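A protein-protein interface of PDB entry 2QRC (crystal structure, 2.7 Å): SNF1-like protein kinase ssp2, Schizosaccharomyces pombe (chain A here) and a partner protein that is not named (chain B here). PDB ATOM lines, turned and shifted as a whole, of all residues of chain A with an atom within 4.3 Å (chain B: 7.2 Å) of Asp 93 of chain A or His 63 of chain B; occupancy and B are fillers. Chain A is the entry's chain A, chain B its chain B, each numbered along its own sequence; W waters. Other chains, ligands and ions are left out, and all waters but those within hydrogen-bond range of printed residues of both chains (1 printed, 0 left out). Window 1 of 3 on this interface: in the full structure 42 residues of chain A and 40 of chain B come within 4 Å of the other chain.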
ATOM      1  N   PHE A  15      13.008 -31.150 -28.369  1.00  0.00           N
ATOM      2  CA  PHE A  15      13.053 -29.733 -28.599  1.00  0.00           C
ATOM      3  C   PHE A  15      14.169 -29.088 -27.824  1.00  0.00           C
ATOM      4  O   PHE A  15      14.532 -29.553 -26.750  1.00  0.00           O
ATOM      5  CB  PHE A  15      11.730 -29.114 -28.255  1.00  0.00           C
ATOM      6  CG  PHE A  15      10.688 -29.328 -29.316  1.00  0.00           C
ATOM      7  CD1 PHE A  15       9.705 -30.300 -29.162  1.00  0.00           C
ATOM      8  CD2 PHE A  15      10.694 -28.555 -30.477  1.00  0.00           C
ATOM      9  CE1 PHE A  15       8.759 -30.500 -30.133  1.00  0.00           C
ATOM     10  CE2 PHE A  15       9.742 -28.739 -31.463  1.00  0.00           C
ATOM     11  CZ  PHE A  15       8.776 -29.718 -31.293  1.00  0.00           C
ATOM     12  N   GLU A  79      13.586 -16.086 -30.666  1.00  0.00           N
ATOM     13  CA  GLU A  79      13.204 -16.085 -29.256  1.00  0.00           C
ATOM     14  C   GLU A  79      13.716 -17.342 -28.550  1.00  0.00           C
ATOM     15  O   GLU A  79      13.529 -18.449 -29.037  1.00  0.00           O
ATOM     16  CB  GLU A  79      11.699 -16.005 -29.120  1.00  0.00           C
ATOM     17  CG  GLU A  79      11.179 -16.232 -27.699  1.00  0.00           C
ATOM     18  CD  GLU A  79       9.629 -16.237 -27.604  1.00  0.00           C
ATOM     19  OE1 GLU A  79       9.042 -15.128 -27.637  1.00  0.00           O
ATOM     20  OE2 GLU A  79       9.010 -17.344 -27.487  1.00  0.00           O
ATOM     21  N   LEU A  80      14.379 -17.159 -27.410  1.00  0.00           N
ATOM     22  CA  LEU A  80      14.853 -18.263 -26.573  1.00  0.00           C
ATOM     23  C   LEU A  80      14.010 -18.276 -25.325  1.00  0.00           C
ATOM     24  O   LEU A  80      13.545 -17.245 -24.882  1.00  0.00           O
ATOM     25  CB  LEU A  80      16.307 -18.070 -26.133  1.00  0.00           C
ATOM     26  CG  LEU A  80      17.487 -17.568 -26.992  1.00  0.00           C
ATOM     27  CD1 LEU A  80      18.106 -18.657 -27.817  1.00  0.00           C
ATOM     28  CD2 LEU A  80      17.153 -16.362 -27.829  1.00  0.00           C
ATOM     29  N   GLN A  81      13.824 -19.451 -24.749  1.00  0.00           N
ATOM     30  CA  GLN A  81      13.078 -19.571 -23.511  1.00  0.00           C
ATOM     31  C   GLN A  81      13.609 -20.720 -22.685  1.00  0.00           C
ATOM     32  O   GLN A  81      13.724 -21.830 -23.188  1.00  0.00           O
ATOM     33  CB  GLN A  81      11.623 -19.849 -23.812  1.00  0.00           C
ATOM     34  CG  GLN A  81      10.785 -20.066 -22.571  1.00  0.00           C
ATOM     35  CD  GLN A  81      10.301 -18.791 -22.025  1.00  0.00           C
ATOM     36  OE1 GLN A  81       9.793 -17.946 -22.761  1.00  0.00           O
ATOM     37  NE2 GLN A  81      10.463 -18.612 -20.737  1.00  0.00           N
ATOM     38  N   TYR A  83      13.077 -23.442 -19.620  1.00  0.00           N
ATOM     39  CA  TYR A  83      12.066 -24.150 -18.856  1.00  0.00           C
ATOM     40  C   TYR A  83      12.733 -25.119 -17.902  1.00  0.00           C
ATOM     41  O   TYR A  83      13.581 -25.880 -18.333  1.00  0.00           O
ATOM     42  CB  TYR A  83      11.171 -24.956 -19.779  1.00  0.00           C
ATOM     43  CG  TYR A  83      10.262 -24.154 -20.669  1.00  0.00           C
ATOM     44  CD1 TYR A  83       9.135 -23.505 -20.146  1.00  0.00           C
ATOM     45  CD2 TYR A  83      10.496 -24.061 -22.044  1.00  0.00           C
ATOM     46  CE1 TYR A  83       8.281 -22.771 -20.973  1.00  0.00           C
ATOM     47  CE2 TYR A  83       9.639 -23.341 -22.872  1.00  0.00           C
ATOM     48  CZ  TYR A  83       8.544 -22.706 -22.328  1.00  0.00           C
ATOM     49  OH  TYR A  83       7.703 -21.985 -23.121  1.00  0.00           O
ATOM     50  N   MET A  91      15.352 -27.179 -20.442  1.00  0.00           N
ATOM     51  CA  MET A  91      15.341 -27.121 -21.877  1.00  0.00           C
ATOM     52  C   MET A  91      15.531 -25.663 -22.216  1.00  0.00           C
ATOM     53  O   MET A  91      14.812 -24.781 -21.721  1.00  0.00           O
ATOM     54  CB  MET A  91      14.005 -27.624 -22.444  1.00  0.00           C
ATOM     55  CG  MET A  91      13.722 -27.135 -23.876  1.00  0.00           C
ATOM     56  SD  MET A  91      12.289 -27.835 -24.743  1.00  0.00           S
ATOM     57  CE  MET A  91      12.404 -29.609 -24.387  1.00  0.00           C
ATOM     58  N   LEU A  92      16.511 -25.392 -23.050  1.00  0.00           N
ATOM     59  CA  LEU A  92      16.606 -24.074 -23.596  1.00  0.00           C
ATOM     60  C   LEU A  92      15.918 -24.116 -24.953  1.00  0.00           C
ATOM     61  O   LEU A  92      16.462 -24.693 -25.888  1.00  0.00           O
ATOM     62  CB  LEU A  92      18.068 -23.667 -23.705  1.00  0.00           C
ATOM     63  CG  LEU A  92      18.213 -22.477 -24.632  1.00  0.00           C
ATOM     64  CD1 LEU A  92      17.833 -21.229 -23.860  1.00  0.00           C
ATOM     65  CD2 LEU A  92      19.618 -22.433 -25.197  1.00  0.00           C
ATOM     66  N   ASP A  93      14.720 -23.546 -25.051  1.00  0.00           N
ATOM     67  CA  ASP A  93      13.909 -23.619 -26.289  1.00  0.00           C
ATOM     68  C   ASP A  93      14.169 -22.442 -27.251  1.00  0.00           C
ATOM     69  O   ASP A  93      14.234 -21.280 -26.843  1.00  0.00           O
ATOM     70  CB  ASP A  93      12.406 -23.783 -25.987  1.00  0.00           C
ATOM     71  CG  ASP A  93      11.502 -23.475 -27.206  1.00  0.00           C
ATOM     72  OD1 ASP A  93      11.263 -24.392 -28.060  1.00  0.00           O
ATOM     73  OD2 ASP A  93      11.013 -22.307 -27.287  1.00  0.00           O
ATOM     74  N   VAL A  94      14.314 -22.773 -28.525  1.00  0.00           N
ATOM     75  CA  VAL A  94      14.704 -21.814 -29.506  1.00  0.00           C
ATOM     76  C   VAL A  94      13.658 -21.818 -30.587  1.00  0.00           C
ATOM     77  O   VAL A  94      13.413 -22.856 -31.192  1.00  0.00           O
ATOM     78  CB  VAL A  94      16.074 -22.178 -30.136  1.00  0.00           C
ATOM     79  CG1 VAL A  94      16.408 -21.223 -31.280  1.00  0.00           C
ATOM     80  CG2 VAL A  94      17.159 -22.117 -29.103  1.00  0.00           C
ATOM     81  N   LYS A  95      13.057 -20.662 -30.840  1.00  0.00           N
ATOM     82  CA  LYS A  95      12.086 -20.543 -31.926  1.00  0.00           C
ATOM     83  C   LYS A  95      12.249 -19.290 -32.821  1.00  0.00           C
ATOM     84  O   LYS A  95      12.816 -18.262 -32.417  1.00  0.00           O
ATOM     85  CB  LYS A  95      10.662 -20.683 -31.392  1.00  0.00           C
ATOM     86  CG  LYS A  95      10.022 -19.412 -30.903  1.00  0.00           C
ATOM     87  CD  LYS A  95       8.946 -18.996 -31.879  1.00  0.00           C
ATOM     88  CE  LYS A  95       7.828 -18.195 -31.191  1.00  0.00           C
ATOM     89  NZ  LYS A  95       6.800 -17.728 -32.176  1.00  0.00           N
ATOM     90  N   LEU B  31       8.404 -26.941 -17.954  1.00  0.00           N
ATOM     91  CA  LEU B  31       8.194 -27.429 -19.319  1.00  0.00           C
ATOM     92  C   LEU B  31       6.705 -27.705 -19.601  1.00  0.00           C
ATOM     93  O   LEU B  31       6.106 -28.558 -18.940  1.00  0.00           O
ATOM     94  CB  LEU B  31       9.019 -28.718 -19.494  1.00  0.00           C
ATOM     95  CG  LEU B  31       9.446 -29.413 -20.804  1.00  0.00           C
ATOM     96  CD1 LEU B  31       8.379 -30.399 -21.292  1.00  0.00           C
ATOM     97  CD2 LEU B  31       9.904 -28.438 -21.928  1.00  0.00           C
ATOM     98  N   HIS B  34       3.391 -29.884 -24.343  1.00  0.00           N
ATOM     99  CA  HIS B  34       3.569 -30.062 -25.791  1.00  0.00           C
ATOM    100  C   HIS B  34       5.027 -30.170 -26.315  1.00  0.00           C
ATOM    101  O   HIS B  34       5.237 -30.682 -27.414  1.00  0.00           O
ATOM    102  CB  HIS B  34       2.699 -29.084 -26.616  1.00  0.00           C
ATOM    103  CG  HIS B  34       2.941 -27.634 -26.322  1.00  0.00           C
ATOM    104  ND1 HIS B  34       2.410 -26.993 -25.221  1.00  0.00           N
ATOM    105  CD2 HIS B  34       3.631 -26.691 -27.007  1.00  0.00           C
ATOM    106  CE1 HIS B  34       2.784 -25.724 -25.229  1.00  0.00           C
ATOM    107  NE2 HIS B  34       3.526 -25.516 -26.303  1.00  0.00           N
ATOM    108  N   LEU B  35       6.028 -29.740 -25.544  1.00  0.00           N
ATOM    109  CA  LEU B  35       7.431 -29.867 -25.996  1.00  0.00           C
ATOM    110  C   LEU B  35       8.085 -31.152 -25.513  1.00  0.00           C
ATOM    111  O   LEU B  35       9.294 -31.329 -25.586  1.00  0.00           O
ATOM    112  CB  LEU B  35       8.267 -28.649 -25.582  1.00  0.00           C
ATOM    113  CG  LEU B  35       7.798 -27.296 -26.112  1.00  0.00           C
ATOM    114  CD1 LEU B  35       8.378 -26.169 -25.279  1.00  0.00           C
ATOM    115  CD2 LEU B  35       8.148 -27.119 -27.579  1.00  0.00           C
ATOM    116  N   VAL B  59       1.525 -24.790 -33.011  1.00  0.00           N
ATOM    117  CA  VAL B  59       2.228 -24.034 -31.982  1.00  0.00           C
ATOM    118  C   VAL B  59       3.739 -24.188 -32.120  1.00  0.00           C
ATOM    119  O   VAL B  59       4.505 -23.371 -31.610  1.00  0.00           O
ATOM    120  CB  VAL B  59       1.804 -24.475 -30.569  1.00  0.00           C
ATOM    121  CG1 VAL B  59       0.809 -23.486 -29.982  1.00  0.00           C
ATOM    122  CG2 VAL B  59       1.214 -25.876 -30.605  1.00  0.00           C
ATOM    123  N   LEU B  60       4.161 -25.241 -32.813  1.00  0.00           N
ATOM    124  CA  LEU B  60       5.505 -25.777 -32.649  1.00  0.00           C
ATOM    125  C   LEU B  60       6.218 -25.627 -33.981  1.00  0.00           C
ATOM    126  O   LEU B  60       7.394 -25.973 -34.130  1.00  0.00           O
ATOM    127  CB  LEU B  60       5.585 -27.198 -32.102  1.00  0.00           C
ATOM    128  CG  LEU B  60       4.924 -27.383 -30.730  1.00  0.00           C
ATOM    129  CD1 LEU B  60       5.193 -28.772 -30.148  1.00  0.00           C
ATOM    130  CD2 LEU B  60       5.373 -26.298 -29.753  1.00  0.00           C
ATOM    131  N   LEU B  61       5.514 -25.085 -34.954  1.00  0.00           N
ATOM    132  CA  LEU B  61       6.170 -24.601 -36.141  1.00  0.00           C
ATOM    133  C   LEU B  61       7.358 -23.697 -35.760  1.00  0.00           C
ATOM    134  O   LEU B  61       7.217 -22.778 -34.965  1.00  0.00           O
ATOM    135  CB  LEU B  61       5.162 -23.832 -36.971  1.00  0.00           C
ATOM    136  CG  LEU B  61       4.365 -24.570 -38.055  1.00  0.00           C
ATOM    137  CD1 LEU B  61       4.430 -26.078 -37.967  1.00  0.00           C
ATOM    138  CD2 LEU B  61       2.943 -24.077 -38.037  1.00  0.00           C
ATOM    139  N   ASN B  62       8.535 -23.998 -36.292  1.00  0.00           N
ATOM    140  CA  ASN B  62       9.723 -23.157 -36.137  1.00  0.00           C
ATOM    141  C   ASN B  62      10.489 -23.240 -34.828  1.00  0.00           C
ATOM    142  O   ASN B  62      11.383 -22.433 -34.579  1.00  0.00           O
ATOM    143  CB  ASN B  62       9.383 -21.711 -36.469  1.00  0.00           C
ATOM    144  CG  ASN B  62       8.990 -21.534 -37.926  1.00  0.00           C
ATOM    145  OD1 ASN B  62       8.022 -20.782 -38.234  1.00  0.00           O
ATOM    146  ND2 ASN B  62       9.737 -22.220 -38.846  1.00  0.00           N
ATOM    147  N   HIS B  63      10.147 -24.208 -33.990  1.00  0.00           N
ATOM    148  CA  HIS B  63      10.936 -24.492 -32.793  1.00  0.00           C
ATOM    149  C   HIS B  63      12.073 -25.443 -33.151  1.00  0.00           C
ATOM    150  O   HIS B  63      11.840 -26.538 -33.658  1.00  0.00           O
ATOM    151  CB  HIS B  63      10.057 -25.117 -31.703  1.00  0.00           C
ATOM    152  CG  HIS B  63       9.157 -24.148 -30.997  1.00  0.00           C
ATOM    153  ND1 HIS B  63       9.213 -23.941 -29.633  1.00  0.00           N
ATOM    154  CD2 HIS B  63       8.164 -23.350 -31.455  1.00  0.00           C
ATOM    155  CE1 HIS B  63       8.302 -23.051 -29.284  1.00  0.00           C
ATOM    156  NE2 HIS B  63       7.655 -22.673 -30.371  1.00  0.00           N
ATOM    157  N   LEU B  64      13.304 -25.046 -32.884  1.00  0.00           N
ATOM    158  CA  LEU B  64      14.428 -25.942 -33.111  1.00  0.00           C
ATOM    159  C   LEU B  64      14.325 -27.189 -32.233  1.00  0.00           C
ATOM    160  O   LEU B  64      13.935 -27.104 -31.067  1.00  0.00           O
ATOM    161  CB  LEU B  64      15.734 -25.216 -32.837  1.00  0.00           C
ATOM    162  CG  LEU B  64      17.017 -26.033 -32.659  1.00  0.00           C
ATOM    163  CD1 LEU B  64      17.478 -26.764 -33.960  1.00  0.00           C
ATOM    164  CD2 LEU B  64      18.104 -25.110 -32.130  1.00  0.00           C
ATOM    165  N   ALA B  65      14.640 -28.343 -32.817  1.00  0.00           N
ATOM    166  CA  ALA B  65      14.817 -29.587 -32.082  1.00  0.00           C
ATOM    167  C   ALA B  65      16.214 -30.081 -32.393  1.00  0.00           C
ATOM    168  O   ALA B  65      16.799 -29.682 -33.402  1.00  0.00           O
ATOM    169  CB  ALA B  65      13.802 -30.604 -32.519  1.00  0.00           C
ATOM    170  N   ALA B  66      16.748 -30.957 -31.540  1.00  0.00           N
ATOM    171  CA  ALA B  66      18.107 -31.466 -31.704  1.00  0.00           C
ATOM    172  C   ALA B  66      18.131 -32.964 -31.398  1.00  0.00           C
ATOM    173  O   ALA B  66      17.144 -33.489 -30.831  1.00  0.00           O
ATOM    174  CB  ALA B  66      19.051 -30.714 -30.780  1.00  0.00           C
ATOM    175  N   SER B  77      16.718 -29.601 -36.513  1.00  0.00           N
ATOM    176  CA  SER B  77      15.539 -29.542 -37.352  1.00  0.00           C
ATOM    177  C   SER B  77      14.499 -28.576 -36.884  1.00  0.00           C
ATOM    178  O   SER B  77      14.394 -28.301 -35.687  1.00  0.00           O
ATOM    179  CB  SER B  77      14.892 -30.913 -37.490  1.00  0.00           C
ATOM    180  OG  SER B  77      14.769 -31.513 -36.224  1.00  0.00           O
ATOM    181  N   ALA B  78      13.733 -28.070 -37.848  1.00  0.00           N
ATOM    182  CA  ALA B  78      12.523 -27.300 -37.555  1.00  0.00           C
ATOM    183  C   ALA B  78      11.378 -27.689 -38.512  1.00  0.00           C
ATOM    184  O   ALA B  78      11.619 -28.227 -39.588  1.00  0.00           O
ATOM    185  CB  ALA B  78      12.824 -25.814 -37.642  1.00  0.00           C
ATOM    186  N   THR B  79      10.139 -27.420 -38.130  1.00  0.00           N
ATOM    187  CA  THR B  79       9.018 -27.688 -39.016  1.00  0.00           C
ATOM    188  C   THR B  79       8.436 -26.374 -39.458  1.00  0.00           C
ATOM    189  O   THR B  79       8.350 -25.458 -38.658  1.00  0.00           O
ATOM    190  CB  THR B  79       7.942 -28.501 -38.312  1.00  0.00           C
ATOM    191  OG1 THR B  79       8.502 -29.757 -37.919  1.00  0.00           O
ATOM    192  CG2 THR B  79       6.784 -28.752 -39.235  1.00  0.00           C
HETATM  193  O   HOH W   1      13.255 -25.341 -29.279  1.00  0.00           O
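The side-chain carboxylate of Asp 93 of chain A lies within hydrogen-bond range of a ring nitrogen (ND1) of His 63 of chain B (2.6 Å).
O of Val 94 of chain A is in hydrogen-bond range of N of Leu 64 of chain B (2.8 Å).
O of Glu 79 of chain A is in hydrogen-bond range of N of Lys 95 of chain A (2.9 Å).
The backbone carbonyl oxygen of Gln 81 of chain A lies within hydrogen-bond range of the backbone NH of Asp 93 of chain A (2.7 Å).
The backbone carbonyl oxygen of Met 91 of chain A lies within hydrogen-bond range of the backbone NH of Tyr 83 of chain A, 3.0 Å away.
O of Val 59 of chain B lies within hydrogen-bond range of NE2 of His 63 of chain B (3.5 Å).
The backbone carbonyl oxygen of Thr 79 of chain B sits at hydrogen-bond distance from the backbone NH of Asn 62 of chain B (2.8 Å).
The backbone NH (N) of Ala 65 of chain B is in hydrogen-bond range of the backbone carbonyl oxygen (O) of Ser 77 of chain B (2.9 Å).
Among the printed residues, pairs that only touch across the chains: Phe 15 of chain A with Leu 35 of chain B, Phe 15 of chain A with Leu 60 of chain B, Phe 15 of chain A with His 63 of chain B, Phe 15 of chain A with Leu 64 of chain B, Phe 15 of chain A with Ala 65 of chain B, Tyr 83 of chain A with Leu 31 of chain B, Tyr 83 of chain A with Leu 35 of chain B, Met 91 of chain A with Leu 31 of chain B, Met 91 of chain A with Leu 35 of chain B, Val 94 of chain A with Asn 62 of chain B, Val 94 of chain A with His 63 of chain B, Lys 95 of chain A with Asn 62 of chain B and Lys 95 of chain A with His 63 of chain B.
Of chain B, only His 63 (2.6 Å) comes within 4 Å of Asp 93 of chain A.
Printed residues of chain A within 4 Å of His 63 of chain B: Phe 15 (3.6 Å), Asp 93 (2.6 Å), Val 94 (3.4 Å) and Lys 95 (3.7 Å).
Printed residues of chain A within 4 Å of Leu 60 of chain B: Phe 15.
Of the printed residues of chain B, Val 94 of chain A touches Asn 62 (3.97 Å), His 63 (3.4 Å) and Leu 64 (2.8 Å).
Of the printed residues of chain A, Leu 31 of chain B touches Tyr 83 and Met 91.
Ala 78 of chain B touches none of the printed residues of chain A.
The nearest residue of chain B that does not touch Asp 93 of chain A is Leu 35 of chain B (4.2 Å).
The nearest printed residue of chain A that does not touch His 63 of chain B is Glu 79 of chain A (6.0 Å).
Hydrophobic or aromatic side chains of chain B that line the printed part of chain A: Leu 31, Leu 35, Leu 60, His 63 and Leu 64.
Of the 10 printed residues of chain A, 6 touch a printed residue of chain B.
Hydrophobic or aromatic side chains of chain A that line the printed part of chain B: Phe 15, Tyr 83 and Met 91.
Water W1 lies within hydrogen-bond range of the side-chain carboxylate of Asp 93 of chain A (2.5 Å), the backbone carbonyl oxygen of Leu 64 of chain B (2.6 Å) and the backbone NH of Val 94 of chain A (2.9 Å).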
